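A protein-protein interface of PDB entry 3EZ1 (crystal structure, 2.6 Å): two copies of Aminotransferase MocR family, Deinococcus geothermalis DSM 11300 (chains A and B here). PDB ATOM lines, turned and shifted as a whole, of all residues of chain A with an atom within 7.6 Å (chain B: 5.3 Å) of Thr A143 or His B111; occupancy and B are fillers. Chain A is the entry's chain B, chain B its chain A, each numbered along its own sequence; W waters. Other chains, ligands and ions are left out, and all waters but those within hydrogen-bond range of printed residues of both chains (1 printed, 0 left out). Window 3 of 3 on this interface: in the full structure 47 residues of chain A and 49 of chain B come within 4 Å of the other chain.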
ATOM      1  N   THR A 106      32.273  -7.306  20.178  1.00  0.00           N
ATOM      2  CA  THR A 106      32.553  -8.610  19.543  1.00  0.00           C
ATOM      3  C   THR A 106      32.905  -9.675  20.599  1.00  0.00           C
ATOM      4  O   THR A 106      32.469 -10.826  20.470  1.00  0.00           O
ATOM      5  CB  THR A 106      33.672  -8.514  18.459  1.00  0.00           C
ATOM      6  OG1 THR A 106      33.224  -7.683  17.382  1.00  0.00           O
ATOM      7  CG2 THR A 106      34.031  -9.882  17.887  1.00  0.00           C
ATOM      8  N   LEU A 109      29.734 -10.711  22.246  1.00  0.00           N
ATOM      9  CA  LEU A 109      29.008 -11.633  21.350  1.00  0.00           C
ATOM     10  C   LEU A 109      29.613 -13.039  21.335  1.00  0.00           C
ATOM     11  O   LEU A 109      28.882 -14.021  21.485  1.00  0.00           O
ATOM     12  CB  LEU A 109      28.915 -11.058  19.929  1.00  0.00           C
ATOM     13  CG  LEU A 109      27.962  -9.865  19.804  1.00  0.00           C
ATOM     14  CD1 LEU A 109      28.236  -9.141  18.532  1.00  0.00           C
ATOM     15  CD2 LEU A 109      26.490 -10.271  19.881  1.00  0.00           C
ATOM     16  N   ARG A 136      27.500   5.774  12.467  1.00  0.00           N
ATOM     17  CA  ARG A 136      28.504   4.695  12.596  1.00  0.00           C
ATOM     18  C   ARG A 136      28.212   3.731  13.754  1.00  0.00           C
ATOM     19  O   ARG A 136      28.624   2.567  13.690  1.00  0.00           O
ATOM     20  CB  ARG A 136      29.941   5.233  12.707  1.00  0.00           C
ATOM     21  CG  ARG A 136      30.352   6.218  11.607  1.00  0.00           C
ATOM     22  CD  ARG A 136      31.864   6.437  11.548  1.00  0.00           C
ATOM     23  NE  ARG A 136      32.530   5.471  10.670  1.00  0.00           N
ATOM     24  CZ  ARG A 136      32.830   5.644   9.372  1.00  0.00           C
ATOM     25  NH1 ARG A 136      32.545   6.777   8.712  1.00  0.00           N
ATOM     26  NH2 ARG A 136      33.442   4.651   8.712  1.00  0.00           N
ATOM     27  N   HIS A 137      27.539   4.213  14.809  1.00  0.00           N
ATOM     28  CA  HIS A 137      27.107   3.349  15.927  1.00  0.00           C
ATOM     29  C   HIS A 137      26.065   2.317  15.486  1.00  0.00           C
ATOM     30  O   HIS A 137      26.139   1.160  15.897  1.00  0.00           O
ATOM     31  CB  HIS A 137      26.510   4.140  17.106  1.00  0.00           C
ATOM     32  CG  HIS A 137      27.521   4.803  17.988  1.00  0.00           C
ATOM     33  ND1 HIS A 137      27.262   5.983  18.651  1.00  0.00           N
ATOM     34  CD2 HIS A 137      28.783   4.449  18.330  1.00  0.00           C
ATOM     35  CE1 HIS A 137      28.314   6.319  19.373  1.00  0.00           C
ATOM     36  NE2 HIS A 137      29.253   5.409  19.191  1.00  0.00           N
ATOM     37  N   PHE A 138      25.106   2.747  14.662  1.00  0.00           N
ATOM     38  CA  PHE A 138      24.036   1.862  14.167  1.00  0.00           C
ATOM     39  C   PHE A 138      24.617   0.815  13.205  1.00  0.00           C
ATOM     40  O   PHE A 138      24.273  -0.365  13.288  1.00  0.00           O
ATOM     41  CB  PHE A 138      22.908   2.636  13.458  1.00  0.00           C
ATOM     42  CG  PHE A 138      22.423   3.865  14.205  1.00  0.00           C
ATOM     43  CD1 PHE A 138      22.118   3.814  15.572  1.00  0.00           C
ATOM     44  CD2 PHE A 138      22.237   5.075  13.522  1.00  0.00           C
ATOM     45  CE1 PHE A 138      21.667   4.963  16.249  1.00  0.00           C
ATOM     46  CE2 PHE A 138      21.780   6.217  14.192  1.00  0.00           C
ATOM     47  CZ  PHE A 138      21.497   6.160  15.557  1.00  0.00           C
ATOM     48  N   LEU A 139      25.483   1.273  12.297  1.00  0.00           N
ATOM     49  CA  LEU A 139      26.183   0.411  11.333  1.00  0.00           C
ATOM     50  C   LEU A 139      27.041  -0.638  12.044  1.00  0.00           C
ATOM     51  O   LEU A 139      27.035  -1.804  11.647  1.00  0.00           O
ATOM     52  CB  LEU A 139      27.071   1.255  10.409  1.00  0.00           C
ATOM     53  CG  LEU A 139      27.887   0.568   9.310  1.00  0.00           C
ATOM     54  CD1 LEU A 139      26.962  -0.161   8.341  1.00  0.00           C
ATOM     55  CD2 LEU A 139      28.751   1.594   8.580  1.00  0.00           C
ATOM     56  N   LEU A 140      27.766  -0.216  13.085  1.00  0.00           N
ATOM     57  CA  LEU A 140      28.610  -1.114  13.885  1.00  0.00           C
ATOM     58  C   LEU A 140      27.781  -2.190  14.582  1.00  0.00           C
ATOM     59  O   LEU A 140      28.090  -3.376  14.464  1.00  0.00           O
ATOM     60  CB  LEU A 140      29.416  -0.330  14.933  1.00  0.00           C
ATOM     61  CG  LEU A 140      30.361  -1.100  15.871  1.00  0.00           C
ATOM     62  CD1 LEU A 140      31.370  -1.910  15.082  1.00  0.00           C
ATOM     63  CD2 LEU A 140      31.062  -0.142  16.825  1.00  0.00           C
ATOM     64  N   LEU A 141      26.730  -1.768  15.286  1.00  0.00           N
ATOM     65  CA  LEU A 141      25.861  -2.689  16.027  1.00  0.00           C
ATOM     66  C   LEU A 141      25.125  -3.676  15.108  1.00  0.00           C
ATOM     67  O   LEU A 141      25.119  -4.880  15.379  1.00  0.00           O
ATOM     68  CB  LEU A 141      24.888  -1.916  16.930  1.00  0.00           C
ATOM     69  CG  LEU A 141      25.556  -1.174  18.098  1.00  0.00           C
ATOM     70  CD1 LEU A 141      24.603  -0.167  18.725  1.00  0.00           C
ATOM     71  CD2 LEU A 141      26.089  -2.144  19.145  1.00  0.00           C
ATOM     72  N   GLN A 142      24.544  -3.171  14.018  1.00  0.00           N
ATOM     73  CA  GLN A 142      23.853  -4.022  13.025  1.00  0.00           C
ATOM     74  C   GLN A 142      24.798  -4.974  12.270  1.00  0.00           C
ATOM     75  O   GLN A 142      24.367  -6.055  11.863  1.00  0.00           O
ATOM     76  CB  GLN A 142      23.045  -3.177  12.041  1.00  0.00           C
ATOM     77  CG  GLN A 142      21.843  -2.486  12.695  1.00  0.00           C
ATOM     78  CD  GLN A 142      21.074  -1.576  11.746  1.00  0.00           C
ATOM     79  OE1 GLN A 142      21.648  -0.960  10.843  1.00  0.00           O
ATOM     80  NE2 GLN A 142      19.767  -1.478  11.960  1.00  0.00           N
ATOM     81  N   THR A 143      26.061  -4.572  12.077  1.00  0.00           N
ATOM     82  CA  THR A 143      27.077  -5.430  11.440  1.00  0.00           C
ATOM     83  C   THR A 143      27.391  -6.622  12.351  1.00  0.00           C
ATOM     84  O   THR A 143      27.407  -7.757  11.891  1.00  0.00           O
ATOM     85  CB  THR A 143      28.387  -4.658  11.104  1.00  0.00           C
ATOM     86  OG1 THR A 143      28.107  -3.615  10.163  1.00  0.00           O
ATOM     87  CG2 THR A 143      29.445  -5.586  10.497  1.00  0.00           C
ATOM     88  N   LEU A 144      27.602  -6.353  13.640  1.00  0.00           N
ATOM     89  CA  LEU A 144      27.889  -7.401  14.640  1.00  0.00           C
ATOM     90  C   LEU A 144      26.691  -8.317  15.012  1.00  0.00           C
ATOM     91  O   LEU A 144      26.886  -9.321  15.700  1.00  0.00           O
ATOM     92  CB  LEU A 144      28.492  -6.769  15.907  1.00  0.00           C
ATOM     93  CG  LEU A 144      29.809  -5.999  15.758  1.00  0.00           C
ATOM     94  CD1 LEU A 144      30.145  -5.270  17.049  1.00  0.00           C
ATOM     95  CD2 LEU A 144      30.941  -6.918  15.343  1.00  0.00           C
ATOM     96  N   GLY A 145      25.474  -7.967  14.582  1.00  0.00           N
ATOM     97  CA  GLY A 145      24.271  -8.782  14.798  1.00  0.00           C
ATOM     98  C   GLY A 145      23.335  -8.355  15.915  1.00  0.00           C
ATOM     99  O   GLY A 145      22.615  -9.199  16.450  1.00  0.00           O
ATOM    100  N   PHE A 146      23.336  -7.063  16.260  1.00  0.00           N
ATOM    101  CA  PHE A 146      22.444  -6.505  17.285  1.00  0.00           C
ATOM    102  C   PHE A 146      21.225  -5.886  16.620  1.00  0.00           C
ATOM    103  O   PHE A 146      21.370  -5.153  15.638  1.00  0.00           O
ATOM    104  CB  PHE A 146      23.114  -5.387  18.095  1.00  0.00           C
ATOM    105  CG  PHE A 146      24.151  -5.858  19.066  1.00  0.00           C
ATOM    106  CD1 PHE A 146      23.771  -6.319  20.326  1.00  0.00           C
ATOM    107  CD2 PHE A 146      25.511  -5.787  18.756  1.00  0.00           C
ATOM    108  CE1 PHE A 146      24.728  -6.742  21.256  1.00  0.00           C
ATOM    109  CE2 PHE A 146      26.484  -6.207  19.681  1.00  0.00           C
ATOM    110  CZ  PHE A 146      26.091  -6.683  20.935  1.00  0.00           C
ATOM    111  N   THR B 106      37.908 -13.776  12.961  1.00  0.00           N
ATOM    112  CA  THR B 106      36.647 -13.387  13.624  1.00  0.00           C
ATOM    113  C   THR B 106      35.566 -13.045  12.592  1.00  0.00           C
ATOM    114  O   THR B 106      34.411 -13.445  12.770  1.00  0.00           O
ATOM    115  CB  THR B 106      36.831 -12.195  14.605  1.00  0.00           C
ATOM    116  OG1 THR B 106      37.764 -12.556  15.627  1.00  0.00           O
ATOM    117  CG2 THR B 106      35.516 -11.812  15.270  1.00  0.00           C
ATOM    118  N   PHE B 107      35.943 -12.313  11.531  1.00  0.00           N
ATOM    119  CA  PHE B 107      35.003 -11.966  10.438  1.00  0.00           C
ATOM    120  C   PHE B 107      34.512 -13.215   9.695  1.00  0.00           C
ATOM    121  O   PHE B 107      33.352 -13.265   9.279  1.00  0.00           O
ATOM    122  CB  PHE B 107      35.583 -10.968   9.415  1.00  0.00           C
ATOM    123  CG  PHE B 107      36.060  -9.650  10.003  1.00  0.00           C
ATOM    124  CD1 PHE B 107      35.343  -8.987  11.018  1.00  0.00           C
ATOM    125  CD2 PHE B 107      37.203  -9.027   9.480  1.00  0.00           C
ATOM    126  CE1 PHE B 107      35.800  -7.758  11.540  1.00  0.00           C
ATOM    127  CE2 PHE B 107      37.663  -7.796   9.992  1.00  0.00           C
ATOM    128  CZ  PHE B 107      36.959  -7.160  11.017  1.00  0.00           C
ATOM    129  N   ALA B 108      35.405 -14.196   9.522  1.00  0.00           N
ATOM    130  CA  ALA B 108      35.053 -15.504   8.945  1.00  0.00           C
ATOM    131  C   ALA B 108      34.042 -16.243   9.849  1.00  0.00           C
ATOM    132  O   ALA B 108      33.102 -16.865   9.346  1.00  0.00           O
ATOM    133  CB  ALA B 108      36.305 -16.358   8.725  1.00  0.00           C
ATOM    134  N   LEU B 109      34.230 -16.150  11.171  1.00  0.00           N
ATOM    135  CA  LEU B 109      33.302 -16.759  12.146  1.00  0.00           C
ATOM    136  C   LEU B 109      31.931 -16.064  12.190  1.00  0.00           C
ATOM    137  O   LEU B 109      30.897 -16.736  12.129  1.00  0.00           O
ATOM    138  CB  LEU B 109      33.936 -16.827  13.543  1.00  0.00           C
ATOM    139  CG  LEU B 109      35.058 -17.868  13.652  1.00  0.00           C
ATOM    140  CD1 LEU B 109      35.906 -17.600  14.851  1.00  0.00           C
ATOM    141  CD2 LEU B 109      34.514 -19.299  13.684  1.00  0.00           C
ATOM    142  N   LEU B 110      31.933 -14.732  12.273  1.00  0.00           N
ATOM    143  CA  LEU B 110      30.682 -13.943  12.332  1.00  0.00           C
ATOM    144  C   LEU B 110      29.928 -13.840  11.002  1.00  0.00           C
ATOM    145  O   LEU B 110      28.695 -13.872  11.006  1.00  0.00           O
ATOM    146  CB  LEU B 110      30.923 -12.517  12.880  1.00  0.00           C
ATOM    147  CG  LEU B 110      31.057 -12.325  14.393  1.00  0.00           C
ATOM    148  CD1 LEU B 110      32.131 -13.201  14.991  1.00  0.00           C
ATOM    149  CD2 LEU B 110      31.331 -10.862  14.694  1.00  0.00           C
ATOM    150  N   HIS B 111      30.661 -13.718   9.887  1.00  0.00           N
ATOM    151  CA  HIS B 111      30.070 -13.470   8.546  1.00  0.00           C
ATOM    152  C   HIS B 111      30.360 -14.495   7.440  1.00  0.00           C
ATOM    153  O   HIS B 111      29.547 -14.644   6.522  1.00  0.00           O
ATOM    154  CB  HIS B 111      30.538 -12.094   8.045  1.00  0.00           C
ATOM    155  CG  HIS B 111      30.656 -11.067   9.127  1.00  0.00           C
ATOM    156  ND1 HIS B 111      29.567 -10.531   9.774  1.00  0.00           N
ATOM    157  CD2 HIS B 111      31.747 -10.493   9.684  1.00  0.00           C
ATOM    158  CE1 HIS B 111      29.983  -9.667  10.682  1.00  0.00           C
ATOM    159  NE2 HIS B 111      31.302  -9.626  10.647  1.00  0.00           N
ATOM    160  N   GLY B 112      31.516 -15.159   7.506  1.00  0.00           N
ATOM    161  CA  GLY B 112      31.953 -16.120   6.478  1.00  0.00           C
ATOM    162  C   GLY B 112      32.829 -15.386   5.483  1.00  0.00           C
ATOM    163  O   GLY B 112      32.628 -14.194   5.255  1.00  0.00           O
ATOM    164  N   VAL B 113      33.795 -16.088   4.883  1.00  0.00           N
ATOM    165  CA  VAL B 113      34.687 -15.477   3.876  1.00  0.00           C
ATOM    166  C   VAL B 113      33.931 -15.291   2.542  1.00  0.00           C
ATOM    167  O   VAL B 113      32.757 -15.671   2.428  1.00  0.00           O
ATOM    168  CB  VAL B 113      36.034 -16.242   3.702  1.00  0.00           C
ATOM    169  CG1 VAL B 113      36.736 -16.373   5.045  1.00  0.00           C
ATOM    170  CG2 VAL B 113      35.834 -17.594   3.067  1.00  0.00           C
ATOM    171  N   GLY B 118      27.859 -19.824   4.554  1.00  0.00           N
ATOM    172  CA  GLY B 118      27.378 -19.370   5.862  1.00  0.00           C
ATOM    173  C   GLY B 118      28.522 -18.948   6.780  1.00  0.00           C
ATOM    174  O   GLY B 118      29.693 -19.080   6.394  1.00  0.00           O
ATOM    175  N   PRO B 119      28.198 -18.423   7.989  1.00  0.00           N
ATOM    176  CA  PRO B 119      29.258 -18.064   8.937  1.00  0.00           C
ATOM    177  C   PRO B 119      29.935 -19.328   9.469  1.00  0.00           C
ATOM    178  O   PRO B 119      29.242 -20.312   9.743  1.00  0.00           O
ATOM    179  CB  PRO B 119      28.509 -17.323  10.064  1.00  0.00           C
ATOM    180  CG  PRO B 119      27.145 -17.077   9.565  1.00  0.00           C
ATOM    181  CD  PRO B 119      26.865 -18.132   8.549  1.00  0.00           C
ATOM    182  N   TRP B 273      36.182  -7.457   0.799  1.00  0.00           N
ATOM    183  CA  TRP B 273      35.444  -8.165   1.865  1.00  0.00           C
ATOM    184  C   TRP B 273      35.969  -7.762   3.256  1.00  0.00           C
ATOM    185  O   TRP B 273      35.181  -7.444   4.142  1.00  0.00           O
ATOM    186  CB  TRP B 273      35.518  -9.696   1.671  1.00  0.00           C
ATOM    187  CG  TRP B 273      35.131 -10.488   2.886  1.00  0.00           C
ATOM    188  CD1 TRP B 273      33.873 -10.835   3.268  1.00  0.00           C
ATOM    189  CD2 TRP B 273      36.018 -11.017   3.884  1.00  0.00           C
ATOM    190  NE1 TRP B 273      33.914 -11.550   4.439  1.00  0.00           N
ATOM    191  CE2 TRP B 273      35.215 -11.677   4.845  1.00  0.00           C
ATOM    192  CE3 TRP B 273      37.412 -10.995   4.061  1.00  0.00           C
ATOM    193  CZ2 TRP B 273      35.759 -12.321   5.970  1.00  0.00           C
ATOM    194  CZ3 TRP B 273      37.959 -11.635   5.183  1.00  0.00           C
ATOM    195  CH2 TRP B 273      37.129 -12.288   6.124  1.00  0.00           C
ATOM    196  N   TYR B 277      34.210  -5.094   6.740  1.00  0.00           N
ATOM    197  CA  TYR B 277      34.111  -5.354   8.190  1.00  0.00           C
ATOM    198  C   TYR B 277      35.066  -4.521   9.055  1.00  0.00           C
ATOM    199  O   TYR B 277      34.711  -4.179  10.189  1.00  0.00           O
ATOM    200  CB  TYR B 277      34.174  -6.856   8.486  1.00  0.00           C
ATOM    201  CG  TYR B 277      33.027  -7.576   7.813  1.00  0.00           C
ATOM    202  CD1 TYR B 277      31.717  -7.417   8.284  1.00  0.00           C
ATOM    203  CD2 TYR B 277      33.232  -8.377   6.683  1.00  0.00           C
ATOM    204  CE1 TYR B 277      30.637  -8.047   7.659  1.00  0.00           C
ATOM    205  CE2 TYR B 277      32.152  -9.024   6.048  1.00  0.00           C
ATOM    206  CZ  TYR B 277      30.858  -8.852   6.546  1.00  0.00           C
ATOM    207  OH  TYR B 277      29.784  -9.467   5.948  1.00  0.00           O
ATOM    208  N   ALA B 280      33.353  -1.053   9.087  1.00  0.00           N
ATOM    209  CA  ALA B 280      32.183  -1.025   9.980  1.00  0.00           C
ATOM    210  C   ALA B 280      32.545  -0.689  11.435  1.00  0.00           C
ATOM    211  O   ALA B 280      31.710  -0.140  12.161  1.00  0.00           O
ATOM    212  CB  ALA B 280      31.428  -2.358   9.925  1.00  0.00           C
HETATM  213  O   HOH W   1      30.299   2.110  11.350  1.00  0.00           O
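The backbone carbonyl oxygen of Leu A139 sits at hydrogen-bond distance from the side-chain hydroxyl of Thr A143, at 2.6 Å.
Among the printed residues, pairs that only touch across the chains: Thr A106 with Thr B106 (3.6 Å), Leu A140 with Ala B280 (3.4 Å), Thr A143 with His B111 (3.4 Å), Thr A143 with Tyr B277 (3.7 Å) and Thr A143 with Ala B280 (3.6 Å).
Thr A143 touches just these residues of chain B: His B111, Tyr B277 and Ala B280. His B111 touches just one residue of chain A: Thr A143 (3.4 Å). Gly B112 touches none of the printed residues of chain A. Printed residues of chain B within 4 Å of Thr A106: Thr B106. Of the printed residues of chain B, Leu A140 touches Ala B280 (3.4 Å). Of the printed residues of chain A, Thr B106 touches Thr A106. Of the printed residues of chain A, Ala B280 touches Leu A140 (3.4 Å) and Thr A143 (3.6 Å). Printed residues of chain A within 4 Å of Tyr B277: Thr A143. Trp B273 touches none of the printed residues of chain A. Leu B109 touches none of the printed residues of chain A. The nearest printed residue of chain B that does not touch Thr A143 is Leu B110 (5.7 Å).
Of the 13 printed residues of chain A, 3 touch a printed residue of chain B. Printed residues of chain A that touch a printed residue of chain B: Thr A106, Leu A140 and Thr A143.
Thr B106 touches its own counterpart, Thr A106. Positions printed for both chains: 106 and 109.
Water W1 lies within hydrogen-bond range of the backbone carbonyl oxygen of Ala B280 (2.8 Å) and the backbone carbonyl oxygen of Arg A136 (2.9 Å).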
